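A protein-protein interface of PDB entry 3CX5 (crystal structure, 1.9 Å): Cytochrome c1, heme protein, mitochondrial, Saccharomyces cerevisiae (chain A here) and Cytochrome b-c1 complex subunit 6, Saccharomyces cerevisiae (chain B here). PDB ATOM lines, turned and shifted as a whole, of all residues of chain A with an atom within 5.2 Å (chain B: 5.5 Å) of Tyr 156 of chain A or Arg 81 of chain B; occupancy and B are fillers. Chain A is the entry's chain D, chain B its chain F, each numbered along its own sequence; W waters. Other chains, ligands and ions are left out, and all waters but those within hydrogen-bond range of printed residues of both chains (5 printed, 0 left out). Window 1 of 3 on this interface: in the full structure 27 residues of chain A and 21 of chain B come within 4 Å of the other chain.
Hydrophobic or aromatic side chains of chain B within 4 Å of the printed part of chain A: Leu 77.
O of Thr 135 of chain A is in hydrogen-bond range of NH2 of Arg 81 of chain B (3.0 Å). OD2 of Asp 134 of chain B is in hydrogen-bond range of OH of Tyr 156 of chain A (2.7 Å).
Water W2 lies within hydrogen-bond range of OH of Tyr 13 of chain A (2.5 Å), OG1 of Thr 137 of chain B (2.6 Å) and OD1 of Asp 134 of chain B (2.9 Å). Water W1 lies within hydrogen-bond range of the side-chain hydroxyl of Thr 135 of chain A, the backbone carbonyl oxygen of Ser 132 of chain A, the guanidinium group of Arg 81 of chain B and the backbone NH of Gly 136 of chain A. Water W4 lies within hydrogen-bond range of OH of Tyr 13 of chain A (2.7 Å), OG of Ser 132 of chain A (3.1 Å), OH of Tyr 156 of chain A (3.1 Å) and OD1 of Asp 134 of chain B (3.3 Å). Water W3 lies within hydrogen-bond range of the side-chain amide nitrogen (NE2) of Gln 130 of chain B, the side-chain hydroxyl (OH) of Tyr 156 of chain A and the guanidinium group (NH1) of Arg 81 of chain B. Water W5 lies within hydrogen-bond range of the backbone carbonyl oxygen of His 9 of chain A (2.7 Å) and the side-chain carboxylate of Asp 134 of chain B (2.8 Å).
The backbone NH (N) of Leu 8 of chain A sits at hydrogen-bond distance from the backbone carbonyl oxygen (O) of Pro 155 of chain A. N of Tyr 156 of chain A lies within hydrogen-bond range of OD1 of Asn 154 of chain A (3.1 Å). The side-chain carboxylate of Asp 134 of chain B is in salt-bridge range of the guanidinium group of Arg 81 of chain B (3.7 Å).
Among the printed residues, merely in contact across the chains: Leu 8 of chain A with Gln 130 of chain B (3.6 Å), Leu 8 of chain A with Asp 134 of chain B (3.8 Å), Pro 11 of chain A with Asp 134 of chain B (3.8 Å), Thr 135 of chain A with Leu 77 of chain B (3.6 Å) and Tyr 156 of chain A with Arg 81 of chain B (3.6 Å).
Printed residues of chain B within 4 Å of Leu 8 of chain A: Gln 130 (3.6 Å) and Asp 134 (3.8 Å). Of the printed residues of chain B, Pro 11 of chain A touches Asp 134 (3.8 Å). Printed residues of chain B within 4 Å of Thr 135 of chain A: Leu 77 (3.6 Å) and Arg 81 (3.0 Å). Pro 155 of chain A touches none of the printed residues of chain B. Arg 81 of chain B touches just these residues of chain A: Thr 135 and Tyr 156. Printed residues of chain A within 4 Å of Gln 130 of chain B: Leu 8. Printed residues of chain A within 4 Å of Asp 134 of chain B: Leu 8 (3.8 Å), Pro 11 (3.8 Å) and Tyr 156 (2.7 Å). The nearest residue of chain B that does not touch Tyr 156 of chain A is Gln 130 of chain B (4.2 Å). The nearest residue of chain A that does not touch Arg 81 of chain B is Gly 136 of chain A (4.6 Å). The nearest printed residue of chain B that does not touch Pro 11 of chain A is Thr 137 of chain B (6.3 Å).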
ATOM      1  N   GLY A   7       1.516 -14.150 -22.668  1.00  0.00           N
ATOM      2  CA  GLY A   7       0.427 -14.073 -23.618  1.00  0.00           C
ATOM      3  C   GLY A   7      -0.859 -14.327 -22.861  1.00  0.00           C
ATOM      4  O   GLY A   7      -0.871 -15.060 -21.871  1.00  0.00           O
ATOM      5  N   LEU A   8      -1.944 -13.714 -23.318  1.00  0.00           N
ATOM      6  CA  LEU A   8      -3.251 -13.867 -22.684  1.00  0.00           C
ATOM      7  C   LEU A   8      -3.730 -15.310 -22.823  1.00  0.00           C
ATOM      8  O   LEU A   8      -3.692 -15.883 -23.912  1.00  0.00           O
ATOM      9  CB  LEU A   8      -4.266 -12.929 -23.355  1.00  0.00           C
ATOM     10  CG  LEU A   8      -5.393 -12.261 -22.554  1.00  0.00           C
ATOM     11  CD1 LEU A   8      -6.591 -12.090 -23.465  1.00  0.00           C
ATOM     12  CD2 LEU A   8      -5.782 -13.053 -21.322  1.00  0.00           C
ATOM     13  N   HIS A   9      -4.196 -15.885 -21.722  1.00  0.00           N
ATOM     14  CA  HIS A   9      -4.701 -17.253 -21.734  1.00  0.00           C
ATOM     15  C   HIS A   9      -5.864 -17.390 -22.719  1.00  0.00           C
ATOM     16  O   HIS A   9      -6.740 -16.524 -22.780  1.00  0.00           O
ATOM     17  CB  HIS A   9      -5.166 -17.653 -20.333  1.00  0.00           C
ATOM     18  CG  HIS A   9      -5.740 -19.034 -20.257  1.00  0.00           C
ATOM     19  ND1 HIS A   9      -7.097 -19.272 -20.176  1.00  0.00           N
ATOM     20  CD2 HIS A   9      -5.143 -20.249 -20.251  1.00  0.00           C
ATOM     21  CE1 HIS A   9      -7.310 -20.575 -20.125  1.00  0.00           C
ATOM     22  NE2 HIS A   9      -6.141 -21.191 -20.170  1.00  0.00           N
ATOM     23  N   ALA A  10      -5.835 -18.451 -23.521  1.00  0.00           N
ATOM     24  CA  ALA A  10      -6.894 -18.709 -24.487  1.00  0.00           C
ATOM     25  C   ALA A  10      -8.018 -19.442 -23.765  1.00  0.00           C
ATOM     26  O   ALA A  10      -7.803 -20.511 -23.196  1.00  0.00           O
ATOM     27  CB  ALA A  10      -6.372 -19.545 -25.644  1.00  0.00           C
ATOM     28  N   PRO A  11      -9.232 -18.870 -23.779  1.00  0.00           N
ATOM     29  CA  PRO A  11     -10.411 -19.454 -23.124  1.00  0.00           C
ATOM     30  C   PRO A  11     -10.877 -20.739 -23.806  1.00  0.00           C
ATOM     31  O   PRO A  11     -10.538 -20.998 -24.957  1.00  0.00           O
ATOM     32  CB  PRO A  11     -11.446 -18.340 -23.254  1.00  0.00           C
ATOM     33  CG  PRO A  11     -11.104 -17.733 -24.586  1.00  0.00           C
ATOM     34  CD  PRO A  11      -9.593 -17.629 -24.494  1.00  0.00           C
ATOM     35  N   TYR A  13     -13.502 -22.824 -25.659  1.00  0.00           N
ATOM     36  CA  TYR A  13     -14.718 -22.782 -26.456  1.00  0.00           C
ATOM     37  C   TYR A  13     -15.323 -24.172 -26.526  1.00  0.00           C
ATOM     38  O   TYR A  13     -14.639 -25.171 -26.282  1.00  0.00           O
ATOM     39  CB  TYR A  13     -14.422 -22.253 -27.855  1.00  0.00           C
ATOM     40  CG  TYR A  13     -14.115 -20.786 -27.852  1.00  0.00           C
ATOM     41  CD1 TYR A  13     -15.143 -19.846 -27.899  1.00  0.00           C
ATOM     42  CD2 TYR A  13     -12.808 -20.327 -27.743  1.00  0.00           C
ATOM     43  CE1 TYR A  13     -14.878 -18.492 -27.836  1.00  0.00           C
ATOM     44  CE2 TYR A  13     -12.534 -18.969 -27.676  1.00  0.00           C
ATOM     45  CZ  TYR A  13     -13.576 -18.060 -27.724  1.00  0.00           C
ATOM     46  OH  TYR A  13     -13.319 -16.716 -27.671  1.00  0.00           O
ATOM     47  N   TYR A 129      -6.407 -21.694 -28.865  1.00  0.00           N
ATOM     48  CA  TYR A 129      -5.388 -20.699 -29.168  1.00  0.00           C
ATOM     49  C   TYR A 129      -5.501 -20.152 -30.591  1.00  0.00           C
ATOM     50  O   TYR A 129      -5.460 -18.934 -30.790  1.00  0.00           O
ATOM     51  CB  TYR A 129      -3.984 -21.264 -28.969  1.00  0.00           C
ATOM     52  CG  TYR A 129      -2.921 -20.338 -29.506  1.00  0.00           C
ATOM     53  CD1 TYR A 129      -2.615 -19.148 -28.846  1.00  0.00           C
ATOM     54  CD2 TYR A 129      -2.258 -20.623 -30.703  1.00  0.00           C
ATOM     55  CE1 TYR A 129      -1.679 -18.261 -29.366  1.00  0.00           C
ATOM     56  CE2 TYR A 129      -1.320 -19.743 -31.231  1.00  0.00           C
ATOM     57  CZ  TYR A 129      -1.037 -18.563 -30.554  1.00  0.00           C
ATOM     58  OH  TYR A 129      -0.103 -17.688 -31.054  1.00  0.00           O
ATOM     59  N   SER A 132      -8.631 -17.971 -30.819  1.00  0.00           N
ATOM     60  CA  SER A 132      -8.448 -16.740 -30.057  1.00  0.00           C
ATOM     61  C   SER A 132      -7.507 -15.757 -30.745  1.00  0.00           C
ATOM     62  O   SER A 132      -7.726 -14.543 -30.710  1.00  0.00           O
ATOM     63  CB  SER A 132      -7.950 -17.042 -28.645  1.00  0.00           C
ATOM     64  OG  SER A 132      -8.910 -17.783 -27.906  1.00  0.00           O
ATOM     65  N   LEU A 133      -6.468 -16.286 -31.386  1.00  0.00           N
ATOM     66  CA  LEU A 133      -5.492 -15.460 -32.086  1.00  0.00           C
ATOM     67  C   LEU A 133      -6.161 -14.760 -33.271  1.00  0.00           C
ATOM     68  O   LEU A 133      -6.083 -13.537 -33.415  1.00  0.00           O
ATOM     69  CB  LEU A 133      -4.341 -16.339 -32.590  1.00  0.00           C
ATOM     70  CG  LEU A 133      -3.142 -15.629 -33.224  1.00  0.00           C
ATOM     71  CD1 LEU A 133      -2.412 -14.819 -32.166  1.00  0.00           C
ATOM     72  CD2 LEU A 133      -2.199 -16.658 -33.843  1.00  0.00           C
ATOM     73  N   THR A 135      -9.279 -14.134 -33.837  1.00  0.00           N
ATOM     74  CA  THR A 135     -10.355 -13.218 -33.461  1.00  0.00           C
ATOM     75  C   THR A 135      -9.948 -12.241 -32.363  1.00  0.00           C
ATOM     76  O   THR A 135     -10.781 -11.482 -31.876  1.00  0.00           O
ATOM     77  CB  THR A 135     -11.596 -13.998 -32.961  1.00  0.00           C
ATOM     78  OG1 THR A 135     -11.247 -14.785 -31.814  1.00  0.00           O
ATOM     79  CG2 THR A 135     -12.139 -14.913 -34.049  1.00  0.00           C
ATOM     80  N   GLY A 136      -8.670 -12.231 -32.002  1.00  0.00           N
ATOM     81  CA  GLY A 136      -8.224 -11.367 -30.919  1.00  0.00           C
ATOM     82  C   GLY A 136      -7.388 -10.151 -31.235  1.00  0.00           C
ATOM     83  O   GLY A 136      -6.656  -9.666 -30.368  1.00  0.00           O
ATOM     84  N   ASN A 154      -1.479  -8.418 -30.691  1.00  0.00           N
ATOM     85  CA  ASN A 154      -2.431  -9.485 -30.423  1.00  0.00           C
ATOM     86  C   ASN A 154      -2.062 -10.003 -29.045  1.00  0.00           C
ATOM     87  O   ASN A 154      -0.997 -10.603 -28.858  1.00  0.00           O
ATOM     88  CB  ASN A 154      -2.358 -10.597 -31.469  1.00  0.00           C
ATOM     89  CG  ASN A 154      -3.538 -11.539 -31.384  1.00  0.00           C
ATOM     90  OD1 ASN A 154      -3.814 -12.101 -30.327  1.00  0.00           O
ATOM     91  ND2 ASN A 154      -4.248 -11.713 -32.493  1.00  0.00           N
ATOM     92  N   PRO A 155      -2.949  -9.791 -28.056  1.00  0.00           N
ATOM     93  CA  PRO A 155      -2.722 -10.221 -26.676  1.00  0.00           C
ATOM     94  C   PRO A 155      -2.473 -11.715 -26.471  1.00  0.00           C
ATOM     95  O   PRO A 155      -1.718 -12.087 -25.580  1.00  0.00           O
ATOM     96  CB  PRO A 155      -3.985  -9.736 -25.958  1.00  0.00           C
ATOM     97  CG  PRO A 155      -5.027  -9.900 -27.001  1.00  0.00           C
ATOM     98  CD  PRO A 155      -4.339  -9.327 -28.227  1.00  0.00           C
ATOM     99  N   TYR A 156      -3.088 -12.555 -27.300  1.00  0.00           N
ATOM    100  CA  TYR A 156      -2.937 -14.008 -27.182  1.00  0.00           C
ATOM    101  C   TYR A 156      -1.585 -14.551 -27.647  1.00  0.00           C
ATOM    102  O   TYR A 156      -1.252 -15.703 -27.372  1.00  0.00           O
ATOM    103  CB  TYR A 156      -4.068 -14.726 -27.924  1.00  0.00           C
ATOM    104  CG  TYR A 156      -5.442 -14.360 -27.413  1.00  0.00           C
ATOM    105  CD1 TYR A 156      -6.197 -13.359 -28.036  1.00  0.00           C
ATOM    106  CD2 TYR A 156      -5.978 -14.990 -26.287  1.00  0.00           C
ATOM    107  CE1 TYR A 156      -7.453 -12.995 -27.546  1.00  0.00           C
ATOM    108  CE2 TYR A 156      -7.230 -14.636 -25.791  1.00  0.00           C
ATOM    109  CZ  TYR A 156      -7.960 -13.636 -26.428  1.00  0.00           C
ATOM    110  OH  TYR A 156      -9.194 -13.291 -25.943  1.00  0.00           O
ATOM    111  N   PHE A 157      -0.805 -13.717 -28.330  1.00  0.00           N
ATOM    112  CA  PHE A 157       0.508 -14.116 -28.829  1.00  0.00           C
ATOM    113  C   PHE A 157       1.582 -13.732 -27.809  1.00  0.00           C
ATOM    114  O   PHE A 157       1.575 -12.618 -27.290  1.00  0.00           O
ATOM    115  CB  PHE A 157       0.779 -13.433 -30.173  1.00  0.00           C
ATOM    116  CG  PHE A 157       2.022 -13.923 -30.873  1.00  0.00           C
ATOM    117  CD1 PHE A 157       2.070 -15.202 -31.422  1.00  0.00           C
ATOM    118  CD2 PHE A 157       3.133 -13.097 -31.000  1.00  0.00           C
ATOM    119  CE1 PHE A 157       3.212 -15.652 -32.093  1.00  0.00           C
ATOM    120  CE2 PHE A 157       4.283 -13.540 -31.672  1.00  0.00           C
ATOM    121  CZ  PHE A 157       4.317 -14.821 -32.219  1.00  0.00           C
ATOM    122  N   PRO A 158       2.493 -14.671 -27.473  1.00  0.00           N
ATOM    123  CA  PRO A 158       3.555 -14.378 -26.501  1.00  0.00           C
ATOM    124  C   PRO A 158       4.316 -13.130 -26.920  1.00  0.00           C
ATOM    125  O   PRO A 158       4.780 -13.034 -28.055  1.00  0.00           O
ATOM    126  CB  PRO A 158       4.432 -15.632 -26.565  1.00  0.00           C
ATOM    127  CG  PRO A 158       3.423 -16.709 -26.822  1.00  0.00           C
ATOM    128  CD  PRO A 158       2.540 -16.085 -27.892  1.00  0.00           C
ATOM    129  N   GLN B  76     -20.767 -12.500 -34.169  1.00  0.00           N
ATOM    130  CA  GLN B  76     -21.276 -12.981 -32.890  1.00  0.00           C
ATOM    131  C   GLN B  76     -20.354 -12.764 -31.689  1.00  0.00           C
ATOM    132  O   GLN B  76     -20.836 -12.546 -30.577  1.00  0.00           O
ATOM    133  CB  GLN B  76     -21.678 -14.454 -32.991  1.00  0.00           C
ATOM    134  CG  GLN B  76     -22.732 -14.748 -34.059  1.00  0.00           C
ATOM    135  CD  GLN B  76     -22.143 -15.071 -35.429  1.00  0.00           C
ATOM    136  OE1 GLN B  76     -22.787 -15.721 -36.252  1.00  0.00           O
ATOM    137  NE2 GLN B  76     -20.914 -14.640 -35.669  1.00  0.00           N
ATOM    138  N   LEU B  77     -19.040 -12.841 -31.890  1.00  0.00           N
ATOM    139  CA  LEU B  77     -18.126 -12.618 -30.774  1.00  0.00           C
ATOM    140  C   LEU B  77     -18.101 -11.129 -30.435  1.00  0.00           C
ATOM    141  O   LEU B  77     -18.154 -10.762 -29.264  1.00  0.00           O
ATOM    142  CB  LEU B  77     -16.719 -13.138 -31.083  1.00  0.00           C
ATOM    143  CG  LEU B  77     -15.686 -13.038 -29.949  1.00  0.00           C
ATOM    144  CD1 LEU B  77     -16.221 -13.650 -28.657  1.00  0.00           C
ATOM    145  CD2 LEU B  77     -14.396 -13.726 -30.373  1.00  0.00           C
ATOM    146  N   GLU B  78     -18.041 -10.278 -31.459  1.00  0.00           N
ATOM    147  CA  GLU B  78     -18.046  -8.828 -31.258  1.00  0.00           C
ATOM    148  C   GLU B  78     -19.319  -8.404 -30.530  1.00  0.00           C
ATOM    149  O   GLU B  78     -19.283  -7.560 -29.635  1.00  0.00           O
ATOM    150  CB  GLU B  78     -17.948  -8.088 -32.596  1.00  0.00           C
ATOM    151  CG  GLU B  78     -16.523  -7.784 -33.043  1.00  0.00           C
ATOM    152  CD  GLU B  78     -15.805  -6.820 -32.104  1.00  0.00           C
ATOM    153  OE1 GLU B  78     -16.024  -5.593 -32.228  1.00  0.00           O
ATOM    154  OE2 GLU B  78     -15.024  -7.286 -31.240  1.00  0.00           O
ATOM    155  N   ASP B  79     -20.435  -9.013 -30.919  1.00  0.00           N
ATOM    156  CA  ASP B  79     -21.727  -8.733 -30.308  1.00  0.00           C
ATOM    157  C   ASP B  79     -21.703  -9.120 -28.828  1.00  0.00           C
ATOM    158  O   ASP B  79     -22.047  -8.313 -27.961  1.00  0.00           O
ATOM    159  CB  ASP B  79     -22.828  -9.499 -31.046  1.00  0.00           C
ATOM    160  CG  ASP B  79     -24.143  -9.490 -30.300  1.00  0.00           C
ATOM    161  OD1 ASP B  79     -24.818  -8.436 -30.281  1.00  0.00           O
ATOM    162  OD2 ASP B  79     -24.495 -10.540 -29.718  1.00  0.00           O
ATOM    163  N   LEU B  80     -21.284 -10.354 -28.546  1.00  0.00           N
ATOM    164  CA  LEU B  80     -21.206 -10.845 -27.174  1.00  0.00           C
ATOM    165  C   LEU B  80     -20.255 -10.003 -26.331  1.00  0.00           C
ATOM    166  O   LEU B  80     -20.550  -9.711 -25.174  1.00  0.00           O
ATOM    167  CB  LEU B  80     -20.771 -12.312 -27.146  1.00  0.00           C
ATOM    168  CG  LEU B  80     -21.858 -13.368 -27.358  1.00  0.00           C
ATOM    169  CD1 LEU B  80     -21.231 -14.746 -27.507  1.00  0.00           C
ATOM    170  CD2 LEU B  80     -22.823 -13.353 -26.180  1.00  0.00           C
ATOM    171  N   ARG B  81     -19.128  -9.605 -26.922  1.00  0.00           N
ATOM    172  CA  ARG B  81     -18.128  -8.789 -26.233  1.00  0.00           C
ATOM    173  C   ARG B  81     -18.673  -7.407 -25.877  1.00  0.00           C
ATOM    174  O   ARG B  81     -18.392  -6.882 -24.799  1.00  0.00           O
ATOM    175  CB  ARG B  81     -16.857  -8.648 -27.085  1.00  0.00           C
ATOM    176  CG  ARG B  81     -15.983  -9.901 -27.096  1.00  0.00           C
ATOM    177  CD  ARG B  81     -14.690  -9.722 -27.890  1.00  0.00           C
ATOM    178  NE  ARG B  81     -13.737 -10.793 -27.581  1.00  0.00           N
ATOM    179  CZ  ARG B  81     -12.754 -11.206 -28.384  1.00  0.00           C
ATOM    180  NH1 ARG B  81     -11.948 -12.181 -27.986  1.00  0.00           N
ATOM    181  NH2 ARG B  81     -12.585 -10.670 -29.589  1.00  0.00           N
ATOM    182  N   GLU B  82     -19.442  -6.818 -26.791  1.00  0.00           N
ATOM    183  CA  GLU B  82     -20.029  -5.504 -26.558  1.00  0.00           C
ATOM    184  C   GLU B  82     -21.025  -5.592 -25.396  1.00  0.00           C
ATOM    185  O   GLU B  82     -21.023  -4.748 -24.502  1.00  0.00           O
ATOM    186  CB  GLU B  82     -20.711  -4.985 -27.831  1.00  0.00           C
ATOM    187  CG  GLU B  82     -21.115  -3.513 -27.771  1.00  0.00           C
ATOM    188  CD  GLU B  82     -19.959  -2.591 -27.387  1.00  0.00           C
ATOM    189  OE1 GLU B  82     -18.825  -2.787 -27.888  1.00  0.00           O
ATOM    190  OE2 GLU B  82     -20.188  -1.666 -26.577  1.00  0.00           O
ATOM    191  N   HIS B  83     -21.821  -6.658 -25.381  1.00  0.00           N
ATOM    192  CA  HIS B  83     -22.800  -6.876 -24.325  1.00  0.00           C
ATOM    193  C   HIS B  83     -22.136  -6.903 -22.947  1.00  0.00           C
ATOM    194  O   HIS B  83     -22.567  -6.205 -22.026  1.00  0.00           O
ATOM    195  CB  HIS B  83     -23.553  -8.189 -24.565  1.00  0.00           C
ATOM    196  CG  HIS B  83     -24.477  -8.571 -23.449  1.00  0.00           C
ATOM    197  ND1 HIS B  83     -25.694  -7.959 -23.246  1.00  0.00           N
ATOM    198  CD2 HIS B  83     -24.356  -9.500 -22.471  1.00  0.00           C
ATOM    199  CE1 HIS B  83     -26.284  -8.493 -22.190  1.00  0.00           C
ATOM    200  NE2 HIS B  83     -25.492  -9.431 -21.703  1.00  0.00           N
ATOM    201  N   PHE B  84     -21.061  -7.675 -22.819  1.00  0.00           N
ATOM    202  CA  PHE B  84     -20.373  -7.786 -21.540  1.00  0.00           C
ATOM    203  C   PHE B  84     -19.520  -6.597 -21.117  1.00  0.00           C
ATOM    204  O   PHE B  84     -19.214  -6.447 -19.937  1.00  0.00           O
ATOM    205  CB  PHE B  84     -19.641  -9.123 -21.432  1.00  0.00           C
ATOM    206  CG  PHE B  84     -20.574 -10.281 -21.240  1.00  0.00           C
ATOM    207  CD1 PHE B  84     -21.024 -11.021 -22.327  1.00  0.00           C
ATOM    208  CD2 PHE B  84     -21.061 -10.589 -19.974  1.00  0.00           C
ATOM    209  CE1 PHE B  84     -21.953 -12.053 -22.160  1.00  0.00           C
ATOM    210  CE2 PHE B  84     -21.991 -11.618 -19.792  1.00  0.00           C
ATOM    211  CZ  PHE B  84     -22.437 -12.350 -20.890  1.00  0.00           C
ATOM    212  N   LYS B  85     -19.158  -5.741 -22.068  1.00  0.00           N
ATOM    213  CA  LYS B  85     -18.403  -4.532 -21.737  1.00  0.00           C
ATOM    214  C   LYS B  85     -19.393  -3.542 -21.099  1.00  0.00           C
ATOM    215  O   LYS B  85     -18.991  -2.568 -20.457  1.00  0.00           O
ATOM    216  CB  LYS B  85     -17.833  -3.870 -22.993  1.00  0.00           C
ATOM    217  CG  LYS B  85     -16.649  -4.555 -23.642  1.00  0.00           C
ATOM    218  CD  LYS B  85     -16.239  -3.754 -24.870  1.00  0.00           C
ATOM    219  CE  LYS B  85     -15.281  -4.511 -25.770  1.00  0.00           C
ATOM    220  NZ  LYS B  85     -15.075  -3.773 -27.050  1.00  0.00           N
ATOM    221  N   ASN B  86     -20.685  -3.803 -21.294  1.00  0.00           N
ATOM    222  CA  ASN B  86     -21.748  -2.944 -20.774  1.00  0.00           C
ATOM    223  C   ASN B  86     -22.325  -3.322 -19.407  1.00  0.00           C
ATOM    224  O   ASN B  86     -23.199  -2.626 -18.898  1.00  0.00           O
ATOM    225  CB  ASN B  86     -22.878  -2.815 -21.806  1.00  0.00           C
ATOM    226  CG  ASN B  86     -22.442  -2.078 -23.064  1.00  0.00           C
ATOM    227  OD1 ASN B  86     -21.532  -1.244 -23.029  1.00  0.00           O
ATOM    228  ND2 ASN B  86     -23.094  -2.379 -24.185  1.00  0.00           N
ATOM    229  N   GLN B 130     -10.013  -8.213 -20.730  1.00  0.00           N
ATOM    230  CA  GLN B 130     -10.119  -9.341 -21.647  1.00  0.00           C
ATOM    231  C   GLN B 130     -10.429 -10.675 -20.963  1.00  0.00           C
ATOM    232  O   GLN B 130     -11.245 -11.450 -21.462  1.00  0.00           O
ATOM    233  CB  GLN B 130      -8.847  -9.431 -22.496  1.00  0.00           C
ATOM    234  CG  GLN B 130      -9.120  -9.600 -23.973  1.00  0.00           C
ATOM    235  CD  GLN B 130     -10.257  -8.717 -24.457  1.00  0.00           C
ATOM    236  OE1 GLN B 130     -10.221  -7.494 -24.310  1.00  0.00           O
ATOM    237  NE2 GLN B 130     -11.291  -9.342 -25.013  1.00  0.00           N
ATOM    238  N   LEU B 133     -14.105 -10.712 -20.154  1.00  0.00           N
ATOM    239  CA  LEU B 133     -14.877 -10.894 -21.380  1.00  0.00           C
ATOM    240  C   LEU B 133     -14.814 -12.337 -21.885  1.00  0.00           C
ATOM    241  O   LEU B 133     -15.843 -12.928 -22.201  1.00  0.00           O
ATOM    242  CB  LEU B 133     -14.415  -9.910 -22.466  1.00  0.00           C
ATOM    243  CG  LEU B 133     -14.510  -8.412 -22.130  1.00  0.00           C
ATOM    244  CD1 LEU B 133     -13.877  -7.573 -23.232  1.00  0.00           C
ATOM    245  CD2 LEU B 133     -15.966  -8.001 -21.911  1.00  0.00           C
ATOM    246  N   ASP B 134     -13.611 -12.910 -21.936  1.00  0.00           N
ATOM    247  CA  ASP B 134     -13.439 -14.293 -22.390  1.00  0.00           C
ATOM    248  C   ASP B 134     -14.193 -15.274 -21.497  1.00  0.00           C
ATOM    249  O   ASP B 134     -14.871 -16.177 -21.991  1.00  0.00           O
ATOM    250  CB  ASP B 134     -11.958 -14.682 -22.417  1.00  0.00           C
ATOM    251  CG  ASP B 134     -11.198 -14.045 -23.568  1.00  0.00           C
ATOM    252  OD1 ASP B 134     -11.817 -13.719 -24.608  1.00  0.00           O
ATOM    253  OD2 ASP B 134      -9.964 -13.889 -23.436  1.00  0.00           O
ATOM    254  N   THR B 137     -17.815 -14.728 -22.591  1.00  0.00           N
ATOM    255  CA  THR B 137     -18.138 -15.028 -23.984  1.00  0.00           C
ATOM    256  C   THR B 137     -17.775 -16.421 -24.502  1.00  0.00           C
ATOM    257  O   THR B 137     -18.522 -16.995 -25.302  1.00  0.00           O
ATOM    258  CB  THR B 137     -17.552 -13.965 -24.934  1.00  0.00           C
ATOM    259  OG1 THR B 137     -16.126 -13.931 -24.801  1.00  0.00           O
ATOM    260  CG2 THR B 137     -18.117 -12.589 -24.594  1.00  0.00           C
HETATM  261  O   HOH W   1     -10.112 -13.845 -29.639  1.00  0.00           O
HETATM  262  O   HOH W   2     -14.070 -15.226 -25.761  1.00  0.00           O
HETATM  263  O   HOH W   3      -9.740 -10.693 -26.732  1.00  0.00           O
HETATM  264  O   HOH W   4     -10.968 -15.525 -27.255  1.00  0.00           O
HETATM  265  O   HOH W   5      -8.515 -15.077 -21.353  1.00  0.00           O
